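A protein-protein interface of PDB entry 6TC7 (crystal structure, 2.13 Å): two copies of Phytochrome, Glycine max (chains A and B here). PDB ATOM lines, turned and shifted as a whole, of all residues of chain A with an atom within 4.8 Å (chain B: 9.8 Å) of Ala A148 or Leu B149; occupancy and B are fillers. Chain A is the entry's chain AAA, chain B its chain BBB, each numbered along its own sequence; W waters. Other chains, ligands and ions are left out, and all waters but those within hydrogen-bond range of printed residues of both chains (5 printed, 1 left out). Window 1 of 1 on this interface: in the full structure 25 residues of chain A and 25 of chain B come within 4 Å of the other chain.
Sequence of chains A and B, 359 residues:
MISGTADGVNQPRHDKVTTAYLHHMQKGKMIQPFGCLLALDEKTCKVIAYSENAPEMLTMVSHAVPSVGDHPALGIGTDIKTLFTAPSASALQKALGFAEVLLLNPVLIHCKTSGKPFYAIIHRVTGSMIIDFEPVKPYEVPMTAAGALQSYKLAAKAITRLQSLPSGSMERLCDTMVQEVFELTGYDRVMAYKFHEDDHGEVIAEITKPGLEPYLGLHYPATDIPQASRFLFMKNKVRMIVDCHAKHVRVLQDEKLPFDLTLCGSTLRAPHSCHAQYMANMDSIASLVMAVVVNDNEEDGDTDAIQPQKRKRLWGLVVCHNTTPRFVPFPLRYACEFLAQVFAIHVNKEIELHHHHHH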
ATOM      1  N   ASN A 105      -0.471   6.116  23.460  1.00  0.00           N
ATOM      2  CA  ASN A 105      -1.520   5.303  22.830  1.00  0.00           C
ATOM      3  C   ASN A 105      -0.843   4.242  21.922  1.00  0.00           C
ATOM      4  O   ASN A 105       0.314   4.489  21.518  1.00  0.00           O
ATOM      5  CB  ASN A 105      -2.370   6.235  22.013  1.00  0.00           C
ATOM      6  CG  ASN A 105      -3.417   6.936  22.879  1.00  0.00           C
ATOM      7  OD1 ASN A 105      -4.037   6.309  23.684  1.00  0.00           O
ATOM      8  ND2 ASN A 105      -3.701   8.191  22.624  1.00  0.00           N
ATOM      9  N   PRO A 106      -1.503   3.081  21.599  1.00  0.00           N
ATOM     10  CA  PRO A 106      -2.813   2.737  22.134  1.00  0.00           C
ATOM     11  C   PRO A 106      -2.636   1.803  23.303  1.00  0.00           C
ATOM     12  O   PRO A 106      -1.647   1.132  23.267  1.00  0.00           O
ATOM     13  CB  PRO A 106      -3.489   1.956  21.038  1.00  0.00           C
ATOM     14  CG  PRO A 106      -2.317   1.184  20.425  1.00  0.00           C
ATOM     15  CD  PRO A 106      -1.099   2.103  20.604  1.00  0.00           C
ATOM     16  N   MET A 143       0.991 -10.516  18.093  1.00  0.00           N
ATOM     17  CA  MET A 143       1.750  -9.747  17.082  1.00  0.00           C
ATOM     18  C   MET A 143       1.569  -8.217  17.232  1.00  0.00           C
ATOM     19  O   MET A 143       2.123  -7.474  16.413  1.00  0.00           O
ATOM     20  CB  MET A 143       1.361 -10.202  15.672  1.00  0.00           C
ATOM     21  CG  MET A 143       1.728 -11.705  15.425  1.00  0.00           C
ATOM     22  SD  MET A 143       3.440 -12.136  15.877  1.00  0.00           S
ATOM     23  CE  MET A 143       4.313 -11.195  14.624  1.00  0.00           C
ATOM     24  N   THR A 144       0.902  -7.736  18.283  1.00  0.00           N
ATOM     25  CA  THR A 144       0.631  -6.280  18.372  1.00  0.00           C
ATOM     26  C   THR A 144       1.938  -5.462  18.511  1.00  0.00           C
ATOM     27  O   THR A 144       2.116  -4.520  17.790  1.00  0.00           O
ATOM     28  CB  THR A 144      -0.348  -6.011  19.516  1.00  0.00           C
ATOM     29  OG1 THR A 144       0.180  -6.730  20.617  1.00  0.00           O
ATOM     30  CG2 THR A 144      -1.737  -6.553  19.274  1.00  0.00           C
ATOM     31  N   ALA A 145       2.804  -5.756  19.440  1.00  0.00           N
ATOM     32  CA  ALA A 145       4.104  -5.058  19.552  1.00  0.00           C
ATOM     33  C   ALA A 145       4.888  -5.158  18.253  1.00  0.00           C
ATOM     34  O   ALA A 145       5.397  -4.123  17.743  1.00  0.00           O
ATOM     35  CB  ALA A 145       4.876  -5.609  20.694  1.00  0.00           C
ATOM     36  N   ALA A 146       4.941  -6.359  17.672  1.00  0.00           N
ATOM     37  CA  ALA A 146       5.711  -6.592  16.413  1.00  0.00           C
ATOM     38  C   ALA A 146       5.176  -5.768  15.287  1.00  0.00           C
ATOM     39  O   ALA A 146       5.954  -5.100  14.514  1.00  0.00           O
ATOM     40  CB  ALA A 146       5.672  -8.079  15.997  1.00  0.00           C
ATOM     41  N   GLY A 147       3.871  -5.789  15.139  1.00  0.00           N
ATOM     42  CA  GLY A 147       3.247  -4.972  14.078  1.00  0.00           C
ATOM     43  C   GLY A 147       3.502  -3.494  14.316  1.00  0.00           C
ATOM     44  O   GLY A 147       3.744  -2.758  13.383  1.00  0.00           O
ATOM     45  N   ALA A 148       3.469  -3.055  15.561  1.00  0.00           N
ATOM     46  CA  ALA A 148       3.697  -1.615  15.881  1.00  0.00           C
ATOM     47  C   ALA A 148       5.130  -1.242  15.518  1.00  0.00           C
ATOM     48  O   ALA A 148       5.363  -0.268  14.809  1.00  0.00           O
ATOM     49  CB  ALA A 148       3.424  -1.362  17.346  1.00  0.00           C
ATOM     50  N   LEU A 149       6.093  -2.035  15.930  1.00  0.00           N
ATOM     51  CA  LEU A 149       7.529  -1.769  15.536  1.00  0.00           C
ATOM     52  C   LEU A 149       7.695  -1.740  14.015  1.00  0.00           C
ATOM     53  O   LEU A 149       8.412  -0.830  13.490  1.00  0.00           O
ATOM     54  CB  LEU A 149       8.438  -2.786  16.205  1.00  0.00           C
ATOM     55  CG  LEU A 149       8.490  -2.657  17.743  1.00  0.00           C
ATOM     56  CD1 LEU A 149       9.188  -3.840  18.312  1.00  0.00           C
ATOM     57  CD2 LEU A 149       9.219  -1.380  18.147  1.00  0.00           C
ATOM     58  N   GLN A 150       7.081  -2.654  13.288  1.00  0.00           N
ATOM     59  CA  GLN A 150       7.281  -2.712  11.798  1.00  0.00           C
ATOM     60  C   GLN A 150       6.696  -1.462  11.161  1.00  0.00           C
ATOM     61  O   GLN A 150       7.355  -0.875  10.237  1.00  0.00           O
ATOM     62  CB  GLN A 150       6.639  -4.009  11.280  1.00  0.00           C
ATOM     63  CG  GLN A 150       6.668  -4.165   9.753  1.00  0.00           C
ATOM     64  CD  GLN A 150       8.074  -4.453   9.234  1.00  0.00           C
ATOM     65  OE1 GLN A 150       9.100  -4.426   9.972  1.00  0.00           O
ATOM     66  NE2 GLN A 150       8.126  -4.526   7.943  1.00  0.00           N
ATOM     67  N   SER A 151       5.462  -1.047  11.562  1.00  0.00           N
ATOM     68  CA  SER A 151       4.870   0.205  11.072  1.00  0.00           C
ATOM     69  C   SER A 151       5.849   1.390  11.293  1.00  0.00           C
ATOM     70  O   SER A 151       6.137   2.165  10.342  1.00  0.00           O
ATOM     71  CB  SER A 151       3.520   0.438  11.698  1.00  0.00           C
ATOM     72  OG  SER A 151       2.647  -0.599  11.360  1.00  0.00           O
ATOM     73  N   TYR A 152       6.377   1.563  12.492  1.00  0.00           N
ATOM     74  CA  TYR A 152       7.300   2.689  12.766  1.00  0.00           C
ATOM     75  C   TYR A 152       8.603   2.518  11.984  1.00  0.00           C
ATOM     76  O   TYR A 152       9.129   3.501  11.431  1.00  0.00           O
ATOM     77  CB  TYR A 152       7.593   2.852  14.259  1.00  0.00           C
ATOM     78  CG  TYR A 152       7.458   4.305  14.656  1.00  0.00           C
ATOM     79  CD1 TYR A 152       8.440   5.203  14.289  1.00  0.00           C
ATOM     80  CD2 TYR A 152       6.266   4.813  15.189  1.00  0.00           C
ATOM     81  CE1 TYR A 152       8.311   6.558  14.554  1.00  0.00           C
ATOM     82  CE2 TYR A 152       6.106   6.176  15.421  1.00  0.00           C
ATOM     83  CZ  TYR A 152       7.156   7.044  15.127  1.00  0.00           C
ATOM     84  OH  TYR A 152       7.135   8.390  15.246  1.00  0.00           O
ATOM     85  N   PRO A 331      -1.446   1.815  15.109  1.00  0.00           N
ATOM     86  CA  PRO A 331       0.019   1.992  15.084  1.00  0.00           C
ATOM     87  C   PRO A 331       0.496   2.572  13.784  1.00  0.00           C
ATOM     88  O   PRO A 331       1.379   3.415  13.761  1.00  0.00           O
ATOM     89  CB  PRO A 331       0.612   0.613  15.446  1.00  0.00           C
ATOM     90  CG  PRO A 331      -0.442   0.123  16.443  1.00  0.00           C
ATOM     91  CD  PRO A 331      -1.747   0.501  15.708  1.00  0.00           C
ATOM     92  N   TYR A 334      -0.468   6.210  13.577  1.00  0.00           N
ATOM     93  CA  TYR A 334       0.435   6.958  14.437  1.00  0.00           C
ATOM     94  C   TYR A 334       1.761   7.169  13.726  1.00  0.00           C
ATOM     95  O   TYR A 334       2.327   8.253  13.827  1.00  0.00           O
ATOM     96  CB  TYR A 334       0.544   6.211  15.757  1.00  0.00           C
ATOM     97  CG  TYR A 334       1.258   6.987  16.829  1.00  0.00           C
ATOM     98  CD1 TYR A 334       0.738   8.188  17.304  1.00  0.00           C
ATOM     99  CD2 TYR A 334       2.390   6.497  17.448  1.00  0.00           C
ATOM    100  CE1 TYR A 334       1.398   8.934  18.292  1.00  0.00           C
ATOM    101  CE2 TYR A 334       3.051   7.199  18.444  1.00  0.00           C
ATOM    102  CZ  TYR A 334       2.533   8.415  18.891  1.00  0.00           C
ATOM    103  OH  TYR A 334       3.137   9.062  19.939  1.00  0.00           O
ATOM    104  N   LEU B 104       8.884 -10.797  12.142  1.00  0.00           N
ATOM    105  CA  LEU B 104       8.541  -9.607  12.901  1.00  0.00           C
ATOM    106  C   LEU B 104       8.602 -10.012  14.372  1.00  0.00           C
ATOM    107  O   LEU B 104       7.725 -10.656  14.872  1.00  0.00           O
ATOM    108  CB  LEU B 104       7.197  -9.078  12.449  1.00  0.00           C
ATOM    109  CG  LEU B 104       7.066  -8.826  10.928  1.00  0.00           C
ATOM    110  CD1 LEU B 104       5.715  -8.215  10.642  1.00  0.00           C
ATOM    111  CD2 LEU B 104       8.185  -7.920  10.382  1.00  0.00           C
ATOM    112  N   ASN B 105       9.568  -9.465  15.069  1.00  0.00           N
ATOM    113  CA  ASN B 105       9.735  -9.651  16.527  1.00  0.00           C
ATOM    114  C   ASN B 105       9.329  -8.358  17.273  1.00  0.00           C
ATOM    115  O   ASN B 105       9.288  -7.291  16.656  1.00  0.00           O
ATOM    116  CB  ASN B 105      11.192  -9.925  16.838  1.00  0.00           C
ATOM    117  CG  ASN B 105      11.583 -11.363  16.489  1.00  0.00           C
ATOM    118  OD1 ASN B 105      10.865 -12.267  16.869  1.00  0.00           O
ATOM    119  ND2 ASN B 105      12.758 -11.547  15.875  1.00  0.00           N
ATOM    120  N   PRO B 106       9.057  -8.434  18.598  1.00  0.00           N
ATOM    121  CA  PRO B 106       8.966  -9.719  19.331  1.00  0.00           C
ATOM    122  C   PRO B 106       7.527 -10.239  19.403  1.00  0.00           C
ATOM    123  O   PRO B 106       6.652  -9.483  19.161  1.00  0.00           O
ATOM    124  CB  PRO B 106       9.346  -9.308  20.713  1.00  0.00           C
ATOM    125  CG  PRO B 106       8.571  -7.918  20.845  1.00  0.00           C
ATOM    126  CD  PRO B 106       8.677  -7.303  19.459  1.00  0.00           C
ATOM    127  N   TYR B 119       8.247 -11.621  26.138  1.00  0.00           N
ATOM    128  CA  TYR B 119       8.583 -11.355  24.728  1.00  0.00           C
ATOM    129  C   TYR B 119       9.378 -12.577  24.200  1.00  0.00           C
ATOM    130  O   TYR B 119      10.356 -13.011  24.815  1.00  0.00           O
ATOM    131  CB  TYR B 119       9.276 -10.016  24.552  1.00  0.00           C
ATOM    132  CG  TYR B 119       8.407  -8.770  24.483  1.00  0.00           C
ATOM    133  CD1 TYR B 119       7.136  -8.746  23.959  1.00  0.00           C
ATOM    134  CD2 TYR B 119       8.864  -7.598  25.033  1.00  0.00           C
ATOM    135  CE1 TYR B 119       6.426  -7.579  23.845  1.00  0.00           C
ATOM    136  CE2 TYR B 119       8.131  -6.431  25.000  1.00  0.00           C
ATOM    137  CZ  TYR B 119       6.912  -6.407  24.374  1.00  0.00           C
ATOM    138  OH  TYR B 119       6.255  -5.197  24.325  1.00  0.00           O
ATOM    139  N   PRO B 142      -0.709  -4.370  28.851  1.00  0.00           N
ATOM    140  CA  PRO B 142      -1.573  -3.458  28.125  1.00  0.00           C
ATOM    141  C   PRO B 142      -0.838  -2.394  27.301  1.00  0.00           C
ATOM    142  O   PRO B 142      -1.450  -1.815  26.428  1.00  0.00           O
ATOM    143  CB  PRO B 142      -2.382  -2.726  29.276  1.00  0.00           C
ATOM    144  CG  PRO B 142      -2.489  -3.855  30.361  1.00  0.00           C
ATOM    145  CD  PRO B 142      -1.063  -4.506  30.290  1.00  0.00           C
ATOM    146  N   MET B 143       0.343  -2.005  27.746  1.00  0.00           N
ATOM    147  CA  MET B 143       1.150  -0.927  27.153  1.00  0.00           C
ATOM    148  C   MET B 143       2.254  -1.471  26.201  1.00  0.00           C
ATOM    149  O   MET B 143       3.122  -0.694  25.774  1.00  0.00           O
ATOM    150  CB  MET B 143       1.810  -0.141  28.322  1.00  0.00           C
ATOM    151  CG  MET B 143       0.826   0.522  29.280  1.00  0.00           C
ATOM    152  SD  MET B 143      -0.515   1.489  28.554  1.00  0.00           S
ATOM    153  CE  MET B 143       0.307   3.013  28.090  1.00  0.00           C
ATOM    154  N   THR B 144       2.246  -2.733  25.815  1.00  0.00           N
ATOM    155  CA  THR B 144       3.302  -3.215  24.879  1.00  0.00           C
ATOM    156  C   THR B 144       3.276  -2.481  23.532  1.00  0.00           C
ATOM    157  O   THR B 144       4.339  -2.075  23.126  1.00  0.00           O
ATOM    158  CB  THR B 144       3.274  -4.732  24.815  1.00  0.00           C
ATOM    159  OG1 THR B 144       1.962  -5.073  24.378  1.00  0.00           O
ATOM    160  CG2 THR B 144       3.649  -5.236  26.210  1.00  0.00           C
ATOM    161  N   ALA B 145       2.177  -2.366  22.815  1.00  0.00           N
ATOM    162  CA  ALA B 145       2.225  -1.593  21.555  1.00  0.00           C
ATOM    163  C   ALA B 145       2.610  -0.155  21.876  1.00  0.00           C
ATOM    164  O   ALA B 145       3.397   0.475  21.170  1.00  0.00           O
ATOM    165  CB  ALA B 145       0.913  -1.723  20.892  1.00  0.00           C
ATOM    166  N   ALA B 146       2.039   0.429  22.936  1.00  0.00           N
ATOM    167  CA  ALA B 146       2.309   1.848  23.293  1.00  0.00           C
ATOM    168  C   ALA B 146       3.782   2.104  23.576  1.00  0.00           C
ATOM    169  O   ALA B 146       4.354   3.124  23.053  1.00  0.00           O
ATOM    170  CB  ALA B 146       1.470   2.315  24.511  1.00  0.00           C
ATOM    171  N   GLY B 147       4.360   1.290  24.417  1.00  0.00           N
ATOM    172  CA  GLY B 147       5.804   1.402  24.658  1.00  0.00           C
ATOM    173  C   GLY B 147       6.693   1.041  23.465  1.00  0.00           C
ATOM    174  O   GLY B 147       7.705   1.747  23.289  1.00  0.00           O
ATOM    175  N   ALA B 148       6.381   0.055  22.639  1.00  0.00           N
ATOM    176  CA  ALA B 148       7.106  -0.174  21.342  1.00  0.00           C
ATOM    177  C   ALA B 148       7.063   1.080  20.462  1.00  0.00           C
ATOM    178  O   ALA B 148       8.127   1.570  20.044  1.00  0.00           O
ATOM    179  CB  ALA B 148       6.455  -1.289  20.608  1.00  0.00           C
ATOM    180  N   LEU B 149       5.894   1.739  20.347  1.00  0.00           N
ATOM    181  CA  LEU B 149       5.788   2.910  19.433  1.00  0.00           C
ATOM    182  C   LEU B 149       6.676   4.028  20.018  1.00  0.00           C
ATOM    183  O   LEU B 149       7.320   4.779  19.230  1.00  0.00           O
ATOM    184  CB  LEU B 149       4.312   3.339  19.261  1.00  0.00           C
ATOM    185  CG  LEU B 149       3.474   2.378  18.405  1.00  0.00           C
ATOM    186  CD1 LEU B 149       2.013   2.758  18.543  1.00  0.00           C
ATOM    187  CD2 LEU B 149       3.909   2.459  16.920  1.00  0.00           C
ATOM    188  N   GLN B 150       6.611   4.229  21.349  1.00  0.00           N
ATOM    189  CA  GLN B 150       7.308   5.348  21.994  1.00  0.00           C
ATOM    190  C   GLN B 150       8.824   5.170  21.824  1.00  0.00           C
ATOM    191  O   GLN B 150       9.532   6.134  21.558  1.00  0.00           O
ATOM    192  CB  GLN B 150       6.844   5.445  23.461  1.00  0.00           C
ATOM    193  CG  GLN B 150       7.505   6.547  24.327  1.00  0.00           C
ATOM    194  CD  GLN B 150       7.215   7.975  23.906  1.00  0.00           C
ATOM    195  OE1 GLN B 150       7.831   8.881  24.461  1.00  0.00           O
ATOM    196  NE2 GLN B 150       6.367   8.219  22.911  1.00  0.00           N
ATOM    197  N   SER B 151       9.335   3.976  22.030  1.00  0.00           N
ATOM    198  CA  SER B 151      10.781   3.660  21.855  1.00  0.00           C
ATOM    199  C   SER B 151      11.166   3.994  20.420  1.00  0.00           C
ATOM    200  O   SER B 151      12.159   4.665  20.208  1.00  0.00           O
ATOM    201  CB  SER B 151      11.066   2.235  22.242  1.00  0.00           C
ATOM    202  OG  SER B 151      10.826   1.989  23.635  1.00  0.00           O
ATOM    203  N   TYR B 152      10.363   3.650  19.426  1.00  0.00           N
ATOM    204  CA  TYR B 152      10.758   3.903  18.013  1.00  0.00           C
ATOM    205  C   TYR B 152      10.632   5.373  17.711  1.00  0.00           C
ATOM    206  O   TYR B 152      11.491   5.901  17.041  1.00  0.00           O
ATOM    207  CB  TYR B 152       9.998   3.050  17.006  1.00  0.00           C
ATOM    208  CG  TYR B 152      10.868   2.444  15.949  1.00  0.00           C
ATOM    209  CD1 TYR B 152      11.414   3.224  14.939  1.00  0.00           C
ATOM    210  CD2 TYR B 152      11.216   1.096  15.984  1.00  0.00           C
ATOM    211  CE1 TYR B 152      12.375   2.718  14.062  1.00  0.00           C
ATOM    212  CE2 TYR B 152      12.120   0.558  15.083  1.00  0.00           C
ATOM    213  CZ  TYR B 152      12.647   1.368  14.076  1.00  0.00           C
ATOM    214  OH  TYR B 152      13.481   0.844  13.162  1.00  0.00           O
ATOM    215  N   LYS B 153       9.612   6.033  18.240  1.00  0.00           N
ATOM    216  CA  LYS B 153       9.480   7.459  18.031  1.00  0.00           C
ATOM    217  C   LYS B 153      10.696   8.174  18.575  1.00  0.00           C
ATOM    218  O   LYS B 153      11.223   9.121  17.889  1.00  0.00           O
ATOM    219  CB  LYS B 153       8.136   7.918  18.609  1.00  0.00           C
ATOM    220  CG  LYS B 153       7.956   9.424  18.621  1.00  0.00           C
ATOM    221  CD  LYS B 153       6.611   9.820  19.062  1.00  0.00           C
ATOM    222  CE  LYS B 153       6.350  11.285  19.429  1.00  0.00           C
ATOM    223  NZ  LYS B 153       4.973  11.353  20.043  1.00  0.00           N
ATOM    224  N   LEU B 154      11.075   7.884  19.810  1.00  0.00           N
ATOM    225  CA  LEU B 154      12.245   8.576  20.397  1.00  0.00           C
ATOM    226  C   LEU B 154      13.489   8.314  19.543  1.00  0.00           C
ATOM    227  O   LEU B 154      14.329   9.255  19.388  1.00  0.00           O
ATOM    228  CB  LEU B 154      12.456   8.054  21.816  1.00  0.00           C
ATOM    229  CG  LEU B 154      11.407   8.527  22.801  1.00  0.00           C
ATOM    230  CD1 LEU B 154      11.643   8.010  24.211  1.00  0.00           C
ATOM    231  CD2 LEU B 154      11.321  10.058  22.835  1.00  0.00           C
ATOM    232  N   ALA B 155      13.627   7.111  19.000  1.00  0.00           N
ATOM    233  CA  ALA B 155      14.818   6.790  18.182  1.00  0.00           C
ATOM    234  C   ALA B 155      14.715   7.545  16.867  1.00  0.00           C
ATOM    235  O   ALA B 155      15.714   7.997  16.353  1.00  0.00           O
ATOM    236  CB  ALA B 155      14.899   5.293  17.898  1.00  0.00           C
ATOM    237  N   ALA B 156      13.520   7.604  16.301  1.00  0.00           N
ATOM    238  CA  ALA B 156      13.301   8.318  15.036  1.00  0.00           C
ATOM    239  C   ALA B 156      13.619   9.805  15.229  1.00  0.00           C
ATOM    240  O   ALA B 156      14.121  10.434  14.288  1.00  0.00           O
ATOM    241  CB  ALA B 156      11.891   8.080  14.514  1.00  0.00           C
ATOM    242  N   LYS B 157      13.311  10.373  16.393  1.00  0.00           N
ATOM    243  CA  LYS B 157      13.669  11.793  16.621  1.00  0.00           C
ATOM    244  C   LYS B 157      15.192  11.924  16.707  1.00  0.00           C
ATOM    245  O   LYS B 157      15.722  12.845  16.122  1.00  0.00           O
ATOM    246  CB  LYS B 157      12.968  12.323  17.870  1.00  0.00           C
ATOM    247  CG  LYS B 157      11.464  12.407  17.723  1.00  0.00           C
ATOM    248  CD  LYS B 157      10.815  13.275  18.787  1.00  0.00           C
ATOM    249  CE  LYS B 157       9.429  13.770  18.406  1.00  0.00           C
ATOM    250  NZ  LYS B 157       9.018  14.864  19.344  1.00  0.00           N
ATOM    251  N   LEU B 184      18.393   7.882  25.363  1.00  0.00           N
ATOM    252  CA  LEU B 184      17.418   6.806  24.984  1.00  0.00           C
ATOM    253  C   LEU B 184      17.554   5.567  25.878  1.00  0.00           C
ATOM    254  O   LEU B 184      16.566   4.901  26.196  1.00  0.00           O
ATOM    255  CB  LEU B 184      17.742   6.489  23.546  1.00  0.00           C
ATOM    256  CG  LEU B 184      16.749   5.651  22.777  1.00  0.00           C
ATOM    257  CD1 LEU B 184      15.404   6.376  22.684  1.00  0.00           C
ATOM    258  CD2 LEU B 184      17.347   5.442  21.385  1.00  0.00           C
ATOM    259  N   PRO B 331      11.948  -4.042  22.542  1.00  0.00           N
ATOM    260  CA  PRO B 331      11.548  -3.032  21.576  1.00  0.00           C
ATOM    261  C   PRO B 331      12.565  -1.910  21.474  1.00  0.00           C
ATOM    262  O   PRO B 331      12.771  -1.358  20.406  1.00  0.00           O
ATOM    263  CB  PRO B 331      10.119  -2.637  22.013  1.00  0.00           C
ATOM    264  CG  PRO B 331       9.618  -3.915  22.553  1.00  0.00           C
ATOM    265  CD  PRO B 331      10.791  -4.447  23.350  1.00  0.00           C
ATOM    266  N   LEU B 332      13.122  -1.553  22.603  1.00  0.00           N
ATOM    267  CA  LEU B 332      14.063  -0.417  22.608  1.00  0.00           C
ATOM    268  C   LEU B 332      15.395  -0.885  21.973  1.00  0.00           C
ATOM    269  O   LEU B 332      16.037  -0.100  21.253  1.00  0.00           O
ATOM    270  CB  LEU B 332      14.242   0.084  24.041  1.00  0.00           C
ATOM    271  CG  LEU B 332      15.285   1.233  24.202  1.00  0.00           C
ATOM    272  CD1 LEU B 332      14.899   2.449  23.362  1.00  0.00           C
ATOM    273  CD2 LEU B 332      15.526   1.613  25.650  1.00  0.00           C
ATOM    274  N   TYR B 334      15.630  -3.039  19.580  1.00  0.00           N
ATOM    275  CA  TYR B 334      15.294  -3.029  18.161  1.00  0.00           C
ATOM    276  C   TYR B 334      15.419  -1.622  17.590  1.00  0.00           C
ATOM    277  O   TYR B 334      15.931  -1.468  16.488  1.00  0.00           O
ATOM    278  CB  TYR B 334      13.914  -3.610  18.005  1.00  0.00           C
ATOM    279  CG  TYR B 334      13.561  -3.974  16.583  1.00  0.00           C
ATOM    280  CD1 TYR B 334      14.369  -4.867  15.837  1.00  0.00           C
ATOM    281  CD2 TYR B 334      12.431  -3.459  15.961  1.00  0.00           C
ATOM    282  CE1 TYR B 334      14.037  -5.205  14.527  1.00  0.00           C
ATOM    283  CE2 TYR B 334      12.111  -3.758  14.651  1.00  0.00           C
ATOM    284  CZ  TYR B 334      12.897  -4.669  13.944  1.00  0.00           C
ATOM    285  OH  TYR B 334      12.569  -5.008  12.690  1.00  0.00           O
ATOM    286  N   ALA B 335      14.738  -0.636  18.193  1.00  0.00           N
ATOM    287  CA  ALA B 335      14.824   0.766  17.786  1.00  0.00           C
ATOM    288  C   ALA B 335      16.291   1.174  17.730  1.00  0.00           C
ATOM    289  O   ALA B 335      16.597   1.910  16.776  1.00  0.00           O
ATOM    290  CB  ALA B 335      14.048   1.739  18.623  1.00  0.00           C
HETATM  291  O   HOH W   1       4.516   7.296  21.580  1.00  0.00           O
HETATM  292  O   HOH W   2      10.010  -4.676  12.414  1.00  0.00           O
HETATM  293  O   HOH W   3       4.116  -8.485  19.505  1.00  0.00           O
HETATM  294  O   HOH W   4       2.654   5.279  22.353  1.00  0.00           O
HETATM  295  O   HOH W   5       8.629  -6.104  14.263  1.00  0.00           O
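OH of Tyr A334 sits at hydrogen-bond distance from NZ of Lys B153, at 2.9 Å.
Among the printed residues, pairs that only touch across the chains: Met A143 with Leu B104 (3.5 Å), Ala A146 with Leu B104 (3.5 Å), Tyr A152 with Lys B153 (3.5 Å), Pro A106 with Ala B146 (3.6 Å), Ala A146 with Pro B106 (3.6 Å), Tyr A152 with Tyr B152 (3.6 Å), Gln A150 with Leu B104 (3.6 Å), Ala A146 with Asn B105 (3.7 Å), Leu A149 with Ala B148 (3.7 Å), Leu A149 with Pro B106 (3.7 Å), Ala A148 with Leu B149 (3.7 Å), Tyr A152 with Leu B149 (3.8 Å), Asn A105 with Ala B146 (3.8 Å), Pro A106 with Leu B149 (3.8 Å), Leu A149 with Asn B105 (3.8 Å), Asn A105 with Leu B149 (3.8 Å), Leu A149 with Tyr B152 (3.8 Å), Tyr A152 with Ala B156 (3.9 Å), Ala A145 with Tyr B119 (3.9 Å) and Tyr A334 with Leu B149 (3.9 Å).
Printed residues of chain B within 4 Å of Met A143: Leu B104 (3.5 Å).
No residue of chain B comes within 4 Å of Gly A147.
Ala A148 touches one residue of chain B.
No residue of chain B comes within 4 Å of Ser A151.
Of the printed residues of chain A, Ala B146 touches Asn A105 and Pro A106.
Printed residues of chain A within 4 Å of Ala B148: Leu A149 (3.7 Å).
Printed residues of chain A within 4 Å of Leu B149: Asn A105, Pro A106, Ala A148, Tyr A152 and Tyr A334.
Gln B150 touches none of the printed residues of chain A.
Printed residues of chain A within 4 Å of Lys B153: Tyr A152 and Tyr A334.
The nearest printed residue of chain A that does not touch Leu B149 is Pro A331 (4.02 Å).
Of the 25 printed residues of chain B, 10 touch a printed residue of chain A.
Printed residues of chain B that touch a printed residue of chain A: Leu B104, Asn B105, Pro B106, Tyr B119, Ala B146, Ala B148, Leu B149, Tyr B152, Lys B153 and Ala B156.
Printed residues of chain A that touch a printed residue of chain B: Asn A105, Pro A106, Met A143, Ala A145, Ala A146, Ala A148, Leu A149, Gln A150, Tyr A152 and Tyr A334.
Pro A106 touches Leu B149, and with the chains exchanged Leu A149 touches Pro B106.
Ala A148 touches Leu B149, and with the chains exchanged Leu A149 touches Ala B148.
Leu A149 touches Tyr B152, and with the chains exchanged Tyr A152 touches Leu B149.
Tyr A334 touches Leu B149, but with the chains exchanged Leu A149 does not touch Tyr B334 (4.02 Å).
14 positions are printed for both chains.
Water W1 bridges the side-chain amide nitrogen of Gln B150 (2.5 Å) and the side-chain hydroxyl of Tyr A334 (2.8 Å).
Water W2 lies within hydrogen-bond range of OH of Tyr B334 (2.6 Å) and OE1 of Gln A150 (2.6 Å).
Water W4 lies within hydrogen-bond range of the backbone carbonyl oxygen (O) of Asn A105 (2.6 Å) and the backbone carbonyl oxygen (O) of Ala B146 (2.8 Å).
Water W3 lies within hydrogen-bond range of the backbone carbonyl oxygen of Pro B106, the backbone NH of Ala A146 and the backbone NH of Ala A145.
Water W5 bridges O of Asn B105 (2.8 Å) and O of Ala A146 (2.9 Å).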
